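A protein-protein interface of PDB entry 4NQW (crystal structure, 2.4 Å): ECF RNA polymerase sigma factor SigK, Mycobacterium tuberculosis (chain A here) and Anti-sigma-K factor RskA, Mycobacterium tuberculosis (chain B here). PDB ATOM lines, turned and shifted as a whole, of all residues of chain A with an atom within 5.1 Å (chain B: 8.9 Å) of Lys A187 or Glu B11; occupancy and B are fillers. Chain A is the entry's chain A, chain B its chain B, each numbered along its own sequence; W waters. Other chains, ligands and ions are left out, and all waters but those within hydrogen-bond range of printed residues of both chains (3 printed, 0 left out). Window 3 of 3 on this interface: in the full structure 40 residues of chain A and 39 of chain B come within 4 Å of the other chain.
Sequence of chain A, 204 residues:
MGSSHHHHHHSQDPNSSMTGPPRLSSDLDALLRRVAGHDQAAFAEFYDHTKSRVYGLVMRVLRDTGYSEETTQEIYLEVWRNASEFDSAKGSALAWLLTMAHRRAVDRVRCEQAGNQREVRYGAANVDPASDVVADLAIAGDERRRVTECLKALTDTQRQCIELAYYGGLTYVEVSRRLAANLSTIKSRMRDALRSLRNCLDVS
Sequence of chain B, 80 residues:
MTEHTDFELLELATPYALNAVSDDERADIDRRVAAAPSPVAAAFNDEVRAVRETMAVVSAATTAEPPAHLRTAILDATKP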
ATOM      1  N   TYR A 172      -3.982 -19.531  -4.879  1.00  0.00           N
ATOM      2  CA  TYR A 172      -4.011 -20.258  -6.155  1.00  0.00           C
ATOM      3  C   TYR A 172      -5.236 -21.171  -6.266  1.00  0.00           C
ATOM      4  O   TYR A 172      -5.740 -21.404  -7.362  1.00  0.00           O
ATOM      5  CB  TYR A 172      -2.713 -21.046  -6.383  1.00  0.00           C
ATOM      6  CG  TYR A 172      -2.622 -22.365  -5.652  1.00  0.00           C
ATOM      7  CD1 TYR A 172      -2.219 -22.420  -4.322  1.00  0.00           C
ATOM      8  CD2 TYR A 172      -2.919 -23.561  -6.296  1.00  0.00           C
ATOM      9  CE1 TYR A 172      -2.125 -23.626  -3.653  1.00  0.00           C
ATOM     10  CE2 TYR A 172      -2.828 -24.774  -5.633  1.00  0.00           C
ATOM     11  CZ  TYR A 172      -2.429 -24.801  -4.312  1.00  0.00           C
ATOM     12  OH  TYR A 172      -2.336 -26.002  -3.646  1.00  0.00           O
ATOM     13  N   LEU A 183      -6.019 -27.245 -10.259  1.00  0.00           N
ATOM     14  CA  LEU A 183      -4.930 -26.727  -9.424  1.00  0.00           C
ATOM     15  C   LEU A 183      -3.595 -26.852 -10.149  1.00  0.00           C
ATOM     16  O   LEU A 183      -2.772 -25.939 -10.112  1.00  0.00           O
ATOM     17  CB  LEU A 183      -4.859 -27.470  -8.084  1.00  0.00           C
ATOM     18  CG  LEU A 183      -6.090 -27.442  -7.170  1.00  0.00           C
ATOM     19  CD1 LEU A 183      -5.768 -28.102  -5.836  1.00  0.00           C
ATOM     20  CD2 LEU A 183      -6.592 -26.024  -6.945  1.00  0.00           C
ATOM     21  N   SER A 184      -3.396 -27.992 -10.804  1.00  0.00           N
ATOM     22  CA  SER A 184      -2.219 -28.224 -11.634  1.00  0.00           C
ATOM     23  C   SER A 184      -2.049 -27.125 -12.679  1.00  0.00           C
ATOM     24  O   SER A 184      -0.942 -26.637 -12.905  1.00  0.00           O
ATOM     25  CB  SER A 184      -2.330 -29.579 -12.337  1.00  0.00           C
ATOM     26  OG  SER A 184      -1.278 -29.763 -13.269  1.00  0.00           O
ATOM     27  N   THR A 185      -3.158 -26.743 -13.305  1.00  0.00           N
ATOM     28  CA  THR A 185      -3.142 -25.764 -14.389  1.00  0.00           C
ATOM     29  C   THR A 185      -2.753 -24.376 -13.894  1.00  0.00           C
ATOM     30  O   THR A 185      -1.930 -23.714 -14.516  1.00  0.00           O
ATOM     31  CB  THR A 185      -4.510 -25.695 -15.102  1.00  0.00           C
ATOM     32  OG1 THR A 185      -4.925 -27.019 -15.467  1.00  0.00           O
ATOM     33  CG2 THR A 185      -4.428 -24.830 -16.358  1.00  0.00           C
ATOM     34  N   ILE A 186      -3.334 -23.943 -12.777  1.00  0.00           N
ATOM     35  CA  ILE A 186      -3.049 -22.610 -12.237  1.00  0.00           C
ATOM     36  C   ILE A 186      -1.625 -22.528 -11.687  1.00  0.00           C
ATOM     37  O   ILE A 186      -0.963 -21.502 -11.827  1.00  0.00           O
ATOM     38  CB  ILE A 186      -4.062 -22.201 -11.143  1.00  0.00           C
ATOM     39  CG1 ILE A 186      -5.482 -22.136 -11.721  1.00  0.00           C
ATOM     40  CG2 ILE A 186      -3.692 -20.860 -10.518  1.00  0.00           C
ATOM     41  CD1 ILE A 186      -5.663 -21.191 -12.894  1.00  0.00           C
ATOM     42  N   LYS A 187      -1.160 -23.609 -11.070  1.00  0.00           N
ATOM     43  CA  LYS A 187       0.204 -23.661 -10.544  1.00  0.00           C
ATOM     44  C   LYS A 187       1.239 -23.598 -11.667  1.00  0.00           C
ATOM     45  O   LYS A 187       2.232 -22.878 -11.562  1.00  0.00           O
ATOM     46  CB  LYS A 187       0.404 -24.912  -9.688  1.00  0.00           C
ATOM     47  CG  LYS A 187      -0.327 -24.852  -8.353  1.00  0.00           C
ATOM     48  CD  LYS A 187       0.030 -26.028  -7.456  1.00  0.00           C
ATOM     49  CE  LYS A 187      -0.525 -27.339  -7.984  1.00  0.00           C
ATOM     50  NZ  LYS A 187      -0.171 -28.474  -7.091  1.00  0.00           N
ATOM     51  N   SER A 188       0.994 -24.345 -12.741  1.00  0.00           N
ATOM     52  CA  SER A 188       1.844 -24.291 -13.932  1.00  0.00           C
ATOM     53  C   SER A 188       1.802 -22.912 -14.587  1.00  0.00           C
ATOM     54  O   SER A 188       2.823 -22.412 -15.059  1.00  0.00           O
ATOM     55  CB  SER A 188       1.413 -25.348 -14.953  1.00  0.00           C
ATOM     56  OG  SER A 188       1.637 -26.653 -14.458  1.00  0.00           O
ATOM     57  N   ARG A 189       0.618 -22.304 -14.609  1.00  0.00           N
ATOM     58  CA  ARG A 189       0.429 -21.013 -15.265  1.00  0.00           C
ATOM     59  C   ARG A 189       1.091 -19.876 -14.490  1.00  0.00           C
ATOM     60  O   ARG A 189       1.690 -18.982 -15.089  1.00  0.00           O
ATOM     61  CB  ARG A 189      -1.066 -20.728 -15.471  1.00  0.00           C
ATOM     62  CG  ARG A 189      -1.399 -19.841 -16.664  1.00  0.00           C
ATOM     63  CD  ARG A 189      -0.718 -20.312 -17.947  1.00  0.00           C
ATOM     64  NE  ARG A 189      -1.658 -20.492 -19.052  1.00  0.00           N
ATOM     65  CZ  ARG A 189      -2.281 -21.633 -19.347  1.00  0.00           C
ATOM     66  NH1 ARG A 189      -2.085 -22.734 -18.625  1.00  0.00           N
ATOM     67  NH2 ARG A 189      -3.112 -21.677 -20.380  1.00  0.00           N
ATOM     68  N   MET A 190       0.982 -19.912 -13.164  1.00  0.00           N
ATOM     69  CA  MET A 190       1.685 -18.953 -12.309  1.00  0.00           C
ATOM     70  C   MET A 190       3.193 -19.064 -12.501  1.00  0.00           C
ATOM     71  O   MET A 190       3.888 -18.054 -12.580  1.00  0.00           O
ATOM     72  CB  MET A 190       1.345 -19.186 -10.839  1.00  0.00           C
ATOM     73  CG  MET A 190      -0.031 -18.691 -10.439  1.00  0.00           C
ATOM     74  SD  MET A 190      -0.336 -18.964  -8.686  1.00  0.00           S
ATOM     75  CE  MET A 190      -1.920 -18.154  -8.513  1.00  0.00           C
ATOM     76  N   ARG A 191       3.683 -20.298 -12.572  1.00  0.00           N
ATOM     77  CA  ARG A 191       5.094 -20.564 -12.848  1.00  0.00           C
ATOM     78  C   ARG A 191       5.524 -20.005 -14.197  1.00  0.00           C
ATOM     79  O   ARG A 191       6.581 -19.389 -14.306  1.00  0.00           O
ATOM     80  CB  ARG A 191       5.372 -22.067 -12.821  1.00  0.00           C
ATOM     81  CG  ARG A 191       5.466 -22.650 -11.426  1.00  0.00           C
ATOM     82  CD  ARG A 191       5.841 -24.125 -11.458  1.00  0.00           C
ATOM     83  NE  ARG A 191       7.173 -24.339 -12.025  1.00  0.00           N
ATOM     84  CZ  ARG A 191       7.902 -25.442 -11.870  1.00  0.00           C
ATOM     85  NH1 ARG A 191       7.457 -26.464 -11.143  1.00  0.00           N
ATOM     86  NH2 ARG A 191       9.100 -25.518 -12.440  1.00  0.00           N
ATOM     87  N   PHE B   7       9.329 -32.795  -6.333  1.00  0.00           N
ATOM     88  CA  PHE B   7       8.841 -32.498  -7.717  1.00  0.00           C
ATOM     89  C   PHE B   7       7.437 -31.890  -7.681  1.00  0.00           C
ATOM     90  O   PHE B   7       7.186 -30.864  -8.309  1.00  0.00           O
ATOM     91  CB  PHE B   7       8.862 -33.764  -8.584  1.00  0.00           C
ATOM     92  CG  PHE B   7       9.240 -33.511 -10.018  1.00  0.00           C
ATOM     93  CD1 PHE B   7      10.576 -33.384 -10.382  1.00  0.00           C
ATOM     94  CD2 PHE B   7       8.268 -33.404 -11.003  1.00  0.00           C
ATOM     95  CE1 PHE B   7      10.935 -33.153 -11.700  1.00  0.00           C
ATOM     96  CE2 PHE B   7       8.620 -33.173 -12.325  1.00  0.00           C
ATOM     97  CZ  PHE B   7       9.955 -33.047 -12.673  1.00  0.00           C
ATOM     98  N   GLU B   8       6.529 -32.532  -6.950  1.00  0.00           N
ATOM     99  CA  GLU B   8       5.208 -31.956  -6.680  1.00  0.00           C
ATOM    100  C   GLU B   8       5.353 -30.751  -5.762  1.00  0.00           C
ATOM    101  O   GLU B   8       4.725 -29.717  -5.978  1.00  0.00           O
ATOM    102  CB  GLU B   8       4.273 -32.981  -6.028  1.00  0.00           C
ATOM    103  CG  GLU B   8       3.659 -33.983  -6.997  1.00  0.00           C
ATOM    104  CD  GLU B   8       2.502 -33.411  -7.799  1.00  0.00           C
ATOM    105  OE1 GLU B   8       2.328 -33.820  -8.967  1.00  0.00           O
ATOM    106  OE2 GLU B   8       1.760 -32.553  -7.272  1.00  0.00           O
ATOM    107  N   LEU B   9       6.189 -30.897  -4.736  1.00  0.00           N
ATOM    108  CA  LEU B   9       6.461 -29.819  -3.788  1.00  0.00           C
ATOM    109  C   LEU B   9       6.962 -28.549  -4.490  1.00  0.00           C
ATOM    110  O   LEU B   9       6.631 -27.434  -4.082  1.00  0.00           O
ATOM    111  CB  LEU B   9       7.474 -30.295  -2.741  1.00  0.00           C
ATOM    112  CG  LEU B   9       7.885 -29.335  -1.621  1.00  0.00           C
ATOM    113  CD1 LEU B   9       6.683 -28.685  -0.954  1.00  0.00           C
ATOM    114  CD2 LEU B   9       8.722 -30.078  -0.592  1.00  0.00           C
ATOM    115  N   LEU B  10       7.745 -28.728  -5.552  1.00  0.00           N
ATOM    116  CA  LEU B  10       8.243 -27.607  -6.359  1.00  0.00           C
ATOM    117  C   LEU B  10       7.142 -26.780  -7.031  1.00  0.00           C
ATOM    118  O   LEU B  10       7.357 -25.609  -7.353  1.00  0.00           O
ATOM    119  CB  LEU B  10       9.226 -28.105  -7.429  1.00  0.00           C
ATOM    120  CG  LEU B  10      10.716 -28.032  -7.085  1.00  0.00           C
ATOM    121  CD1 LEU B  10      11.196 -26.590  -7.168  1.00  0.00           C
ATOM    122  CD2 LEU B  10      11.020 -28.634  -5.719  1.00  0.00           C
ATOM    123  N   GLU B  11       5.977 -27.387  -7.249  1.00  0.00           N
ATOM    124  CA  GLU B  11       4.846 -26.688  -7.861  1.00  0.00           C
ATOM    125  C   GLU B  11       4.285 -25.601  -6.943  1.00  0.00           C
ATOM    126  O   GLU B  11       3.727 -24.609  -7.416  1.00  0.00           O
ATOM    127  CB  GLU B  11       3.731 -27.673  -8.220  1.00  0.00           C
ATOM    128  CG  GLU B  11       4.112 -28.706  -9.271  1.00  0.00           C
ATOM    129  CD  GLU B  11       3.093 -29.825  -9.392  1.00  0.00           C
ATOM    130  OE1 GLU B  11       1.934 -29.643  -8.954  1.00  0.00           O
ATOM    131  OE2 GLU B  11       3.445 -30.900  -9.926  1.00  0.00           O
ATOM    132  N   LEU B  12       4.436 -25.793  -5.634  1.00  0.00           N
ATOM    133  CA  LEU B  12       3.914 -24.853  -4.646  1.00  0.00           C
ATOM    134  C   LEU B  12       4.834 -23.657  -4.383  1.00  0.00           C
ATOM    135  O   LEU B  12       4.417 -22.701  -3.734  1.00  0.00           O
ATOM    136  CB  LEU B  12       3.613 -25.585  -3.332  1.00  0.00           C
ATOM    137  CG  LEU B  12       2.487 -26.619  -3.427  1.00  0.00           C
ATOM    138  CD1 LEU B  12       2.365 -27.428  -2.144  1.00  0.00           C
ATOM    139  CD2 LEU B  12       1.162 -25.945  -3.751  1.00  0.00           C
ATOM    140  N   ALA B  13       6.060 -23.698  -4.899  1.00  0.00           N
ATOM    141  CA  ALA B  13       7.043 -22.644  -4.644  1.00  0.00           C
ATOM    142  C   ALA B  13       6.580 -21.269  -5.124  1.00  0.00           C
ATOM    143  O   ALA B  13       6.618 -20.301  -4.365  1.00  0.00           O
ATOM    144  CB  ALA B  13       8.377 -23.001  -5.283  1.00  0.00           C
ATOM    145  N   THR B  14       6.143 -21.183  -6.378  1.00  0.00           N
ATOM    146  CA  THR B  14       5.715 -19.904  -6.950  1.00  0.00           C
ATOM    147  C   THR B  14       4.501 -19.327  -6.201  1.00  0.00           C
ATOM    148  O   THR B  14       4.555 -18.180  -5.759  1.00  0.00           O
ATOM    149  CB  THR B  14       5.479 -20.000  -8.479  1.00  0.00           C
ATOM    150  OG1 THR B  14       6.746 -20.074  -9.149  1.00  0.00           O
ATOM    151  CG2 THR B  14       4.722 -18.788  -9.010  1.00  0.00           C
ATOM    152  N   PRO B  15       3.418 -20.116  -6.038  1.00  0.00           N
ATOM    153  CA  PRO B  15       2.292 -19.635  -5.224  1.00  0.00           C
ATOM    154  C   PRO B  15       2.711 -19.204  -3.816  1.00  0.00           C
ATOM    155  O   PRO B  15       2.290 -18.145  -3.349  1.00  0.00           O
ATOM    156  CB  PRO B  15       1.361 -20.846  -5.155  1.00  0.00           C
ATOM    157  CG  PRO B  15       1.660 -21.623  -6.386  1.00  0.00           C
ATOM    158  CD  PRO B  15       3.116 -21.412  -6.676  1.00  0.00           C
ATOM    159  N   TYR B  16       3.538 -20.022  -3.167  1.00  0.00           N
ATOM    160  CA  TYR B  16       4.090 -19.720  -1.842  1.00  0.00           C
ATOM    161  C   TYR B  16       4.813 -18.368  -1.834  1.00  0.00           C
ATOM    162  O   TYR B  16       4.574 -17.539  -0.955  1.00  0.00           O
ATOM    163  CB  TYR B  16       5.055 -20.841  -1.414  1.00  0.00           C
ATOM    164  CG  TYR B  16       5.654 -20.699  -0.030  1.00  0.00           C
ATOM    165  CD1 TYR B  16       6.802 -19.944   0.184  1.00  0.00           C
ATOM    166  CD2 TYR B  16       5.085 -21.344   1.061  1.00  0.00           C
ATOM    167  CE1 TYR B  16       7.353 -19.817   1.448  1.00  0.00           C
ATOM    168  CE2 TYR B  16       5.629 -21.226   2.329  1.00  0.00           C
ATOM    169  CZ  TYR B  16       6.763 -20.461   2.517  1.00  0.00           C
ATOM    170  OH  TYR B  16       7.307 -20.343   3.777  1.00  0.00           O
ATOM    171  N   ALA B  17       5.680 -18.153  -2.824  1.00  0.00           N
ATOM    172  CA  ALA B  17       6.470 -16.919  -2.922  1.00  0.00           C
ATOM    173  C   ALA B  17       5.615 -15.678  -3.181  1.00  0.00           C
ATOM    174  O   ALA B  17       5.981 -14.574  -2.775  1.00  0.00           O
ATOM    175  CB  ALA B  17       7.533 -17.056  -4.002  1.00  0.00           C
ATOM    176  N   LEU B  18       4.479 -15.863  -3.850  1.00  0.00           N
ATOM    177  CA  LEU B  18       3.536 -14.775  -4.094  1.00  0.00           C
ATOM    178  C   LEU B  18       2.561 -14.564  -2.931  1.00  0.00           C
ATOM    179  O   LEU B  18       1.663 -13.725  -3.023  1.00  0.00           O
ATOM    180  CB  LEU B  18       2.740 -15.055  -5.368  1.00  0.00           C
ATOM    181  CG  LEU B  18       3.569 -15.230  -6.639  1.00  0.00           C
ATOM    182  CD1 LEU B  18       2.707 -15.807  -7.752  1.00  0.00           C
ATOM    183  CD2 LEU B  18       4.195 -13.908  -7.055  1.00  0.00           C
ATOM    184  N   ALA B  20       0.370 -16.593  -2.225  1.00  0.00           N
ATOM    185  CA  ALA B  20      -0.863 -17.061  -2.850  1.00  0.00           C
ATOM    186  C   ALA B  20      -1.272 -18.435  -2.314  1.00  0.00           C
ATOM    187  O   ALA B  20      -1.843 -19.248  -3.040  1.00  0.00           O
ATOM    188  CB  ALA B  20      -0.696 -17.109  -4.362  1.00  0.00           C
ATOM    189  N   VAL B  21      -0.965 -18.687  -1.046  1.00  0.00           N
ATOM    190  CA  VAL B  21      -1.471 -19.852  -0.328  1.00  0.00           C
ATOM    191  C   VAL B  21      -2.124 -19.362   0.956  1.00  0.00           C
ATOM    192  O   VAL B  21      -1.785 -18.291   1.466  1.00  0.00           O
ATOM    193  CB  VAL B  21      -0.356 -20.866   0.018  1.00  0.00           C
ATOM    194  CG1 VAL B  21       0.210 -21.501  -1.247  1.00  0.00           C
ATOM    195  CG2 VAL B  21       0.756 -20.214   0.832  1.00  0.00           C
ATOM    196  N   GLU B  25      -2.320 -23.765   4.440  1.00  0.00           N
ATOM    197  CA  GLU B  25      -1.486 -24.442   3.445  1.00  0.00           C
ATOM    198  C   GLU B  25      -0.018 -24.015   3.524  1.00  0.00           C
ATOM    199  O   GLU B  25       0.878 -24.839   3.335  1.00  0.00           O
ATOM    200  CB  GLU B  25      -2.039 -24.219   2.034  1.00  0.00           C
ATOM    201  CG  GLU B  25      -1.292 -24.992   0.954  1.00  0.00           C
ATOM    202  CD  GLU B  25      -2.100 -25.203  -0.319  1.00  0.00           C
ATOM    203  OE1 GLU B  25      -1.634 -25.977  -1.183  1.00  0.00           O
ATOM    204  OE2 GLU B  25      -3.190 -24.605  -0.461  1.00  0.00           O
ATOM    205  N   ILE B  29       3.160 -26.486   3.845  1.00  0.00           N
ATOM    206  CA  ILE B  29       4.305 -26.441   2.938  1.00  0.00           C
ATOM    207  C   ILE B  29       5.602 -26.332   3.734  1.00  0.00           C
ATOM    208  O   ILE B  29       6.520 -27.122   3.522  1.00  0.00           O
ATOM    209  CB  ILE B  29       4.193 -25.272   1.936  1.00  0.00           C
ATOM    210  CG1 ILE B  29       3.066 -25.548   0.934  1.00  0.00           C
ATOM    211  CG2 ILE B  29       5.503 -25.071   1.186  1.00  0.00           C
ATOM    212  CD1 ILE B  29       2.521 -24.309   0.256  1.00  0.00           C
ATOM    213  N   ARG B  32       6.458 -29.418   5.114  1.00  0.00           N
ATOM    214  CA  ARG B  32       6.918 -30.369   4.096  1.00  0.00           C
ATOM    215  C   ARG B  32       8.342 -30.131   3.592  1.00  0.00           C
ATOM    216  O   ARG B  32       9.062 -31.097   3.333  1.00  0.00           O
ATOM    217  CB  ARG B  32       5.962 -30.391   2.906  1.00  0.00           C
ATOM    218  CG  ARG B  32       4.664 -31.134   3.169  1.00  0.00           C
ATOM    219  CD  ARG B  32       3.716 -30.986   1.993  1.00  0.00           C
ATOM    220  NE  ARG B  32       4.242 -31.636   0.794  1.00  0.00           N
ATOM    221  CZ  ARG B  32       3.699 -31.554  -0.419  1.00  0.00           C
ATOM    222  NH1 ARG B  32       2.594 -30.841  -0.627  1.00  0.00           N
ATOM    223  NH2 ARG B  32       4.270 -32.188  -1.438  1.00  0.00           N
ATOM    224  N   ALA B  43      16.085 -26.693  -4.070  1.00  0.00           N
ATOM    225  CA  ALA B  43      15.392 -26.411  -5.328  1.00  0.00           C
ATOM    226  C   ALA B  43      14.153 -25.557  -5.082  1.00  0.00           C
ATOM    227  O   ALA B  43      13.892 -24.606  -5.820  1.00  0.00           O
ATOM    228  CB  ALA B  43      15.008 -27.705  -6.025  1.00  0.00           C
ATOM    229  N   PHE B  44      13.402 -25.908  -4.040  1.00  0.00           N
ATOM    230  CA  PHE B  44      12.212 -25.159  -3.641  1.00  0.00           C
ATOM    231  C   PHE B  44      12.574 -23.730  -3.245  1.00  0.00           C
ATOM    232  O   PHE B  44      11.979 -22.775  -3.739  1.00  0.00           O
ATOM    233  CB  PHE B  44      11.505 -25.868  -2.479  1.00  0.00           C
ATOM    234  CG  PHE B  44      10.257 -25.172  -2.005  1.00  0.00           C
ATOM    235  CD1 PHE B  44       9.016 -25.507  -2.531  1.00  0.00           C
ATOM    236  CD2 PHE B  44      10.321 -24.187  -1.026  1.00  0.00           C
ATOM    237  CE1 PHE B  44       7.864 -24.868  -2.094  1.00  0.00           C
ATOM    238  CE2 PHE B  44       9.173 -23.546  -0.587  1.00  0.00           C
ATOM    239  CZ  PHE B  44       7.943 -23.888  -1.121  1.00  0.00           C
ATOM    240  N   GLU B  47      13.714 -21.561  -6.163  1.00  0.00           N
ATOM    241  CA  GLU B  47      12.470 -21.142  -6.819  1.00  0.00           C
ATOM    242  C   GLU B  47      11.813 -19.963  -6.096  1.00  0.00           C
ATOM    243  O   GLU B  47      11.579 -18.908  -6.693  1.00  0.00           O
ATOM    244  CB  GLU B  47      11.478 -22.313  -6.874  1.00  0.00           C
ATOM    245  CG  GLU B  47      11.349 -22.995  -8.227  1.00  0.00           C
ATOM    246  CD  GLU B  47      10.119 -22.540  -8.989  1.00  0.00           C
ATOM    247  OE1 GLU B  47       9.893 -21.313  -9.079  1.00  0.00           O
ATOM    248  OE2 GLU B  47       9.378 -23.411  -9.491  1.00  0.00           O
ATOM    249  N   VAL B  48      11.516 -20.160  -4.813  1.00  0.00           N
ATOM    250  CA  VAL B  48      10.888 -19.127  -3.990  1.00  0.00           C
ATOM    251  C   VAL B  48      11.674 -17.823  -4.077  1.00  0.00           C
ATOM    252  O   VAL B  48      11.101 -16.773  -4.344  1.00  0.00           O
ATOM    253  CB  VAL B  48      10.758 -19.574  -2.516  1.00  0.00           C
ATOM    254  CG1 VAL B  48      10.484 -18.391  -1.591  1.00  0.00           C
ATOM    255  CG2 VAL B  48       9.656 -20.614  -2.381  1.00  0.00           C
HETATM  256  O   HOH W   1       1.389 -27.849 -11.765  1.00  0.00           O
HETATM  257  O   HOH W   2       1.920 -29.696  -5.707  1.00  0.00           O
HETATM  258  O   HOH W   3       7.695 -29.446 -10.850  1.00  0.00           O
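Water W2 lies within hydrogen-bond range of NZ of Lys A187, O of Glu B8 and OE1 of Glu B11.
Water W1 lies within hydrogen-bond range of the backbone carbonyl oxygen of Ser A184 (2.9 Å), the side-chain hydroxyl of Ser A188 (3.0 Å) and the side-chain carboxylate of Glu B11 (3.4 Å).
Water W3 lies within hydrogen-bond range of O of Phe B7 (3.0 Å) and NH1 of Arg A191 (3.0 Å).
Printed residues of chain B that touch a printed residue of chain A: Leu B10, Glu B11, Leu B12, Thr B14, Pro B15, Ala B20, Val B21, Glu B25 and Glu B47.
Hydrophobic or aromatic side chains of chain B that line the printed part of chain A: Leu B12, Pro B15 and Val B21.
Along chain A the printed residues that touch a printed residue of chain B span positions 172 to 191.
Lys A187 touches just these residues of chain B: Glu B11 and Leu B12.
Glu B11 touches just one residue of chain A: Lys A187.
No residue of chain B comes within 4 Å of Ser A188.
Printed residues of chain B within 4 Å of Met A190: Thr B14 (3.7 Å).
Printed residues of chain B within 4 Å of Arg A191: Leu B10, Thr B14 and Glu B47.
Printed residues of chain A within 4 Å of Thr B14: Met A190 (3.7 Å) and Arg A191 (3.7 Å).
Printed residues of chain A within 4 Å of Pro B15: Tyr A172.
Of the printed residues of chain A, Ala B20 touches Tyr A172 (2.8 Å).
The nearest residue of chain A that does not touch Glu B11 is Arg A191 (4.2 Å).
O of Ala B20 sits at hydrogen-bond distance from N of Tyr A172, at 2.8 Å.
OE1 of Glu B25 is in hydrogen-bond range of OH of Tyr A172, 2.6 Å away.
The side-chain amino group (NZ) of Lys A187 lies within salt-bridge range of the side-chain carboxylate (OE1) of Glu B11, at 3.0 Å.
The guanidinium group (NE) of Arg A191 lies within salt-bridge range of the side-chain carboxylate (OE2) of Glu B47 (3.5 Å).
The side-chain hydroxyl (OG1) of Thr B14 lies within hydrogen-bond range of the side-chain carboxylate (OE1) of Glu B47 (3.4 Å).
O of Pro B15 sits at hydrogen-bond distance from N of Ala B20 (2.7 Å).
Among the printed residues, pairs that only touch across the chains: Tyr A172 with Leu B12 (3.5 Å), Arg A191 with Thr B14 (3.7 Å), Met A190 with Thr B14 (3.7 Å), Lys A187 with Leu B12 (3.9 Å), Arg A191 with Leu B10 (3.9 Å), Tyr A172 with Val B21 (3.97 Å) and Tyr A172 with Pro B15 (3.998 Å).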
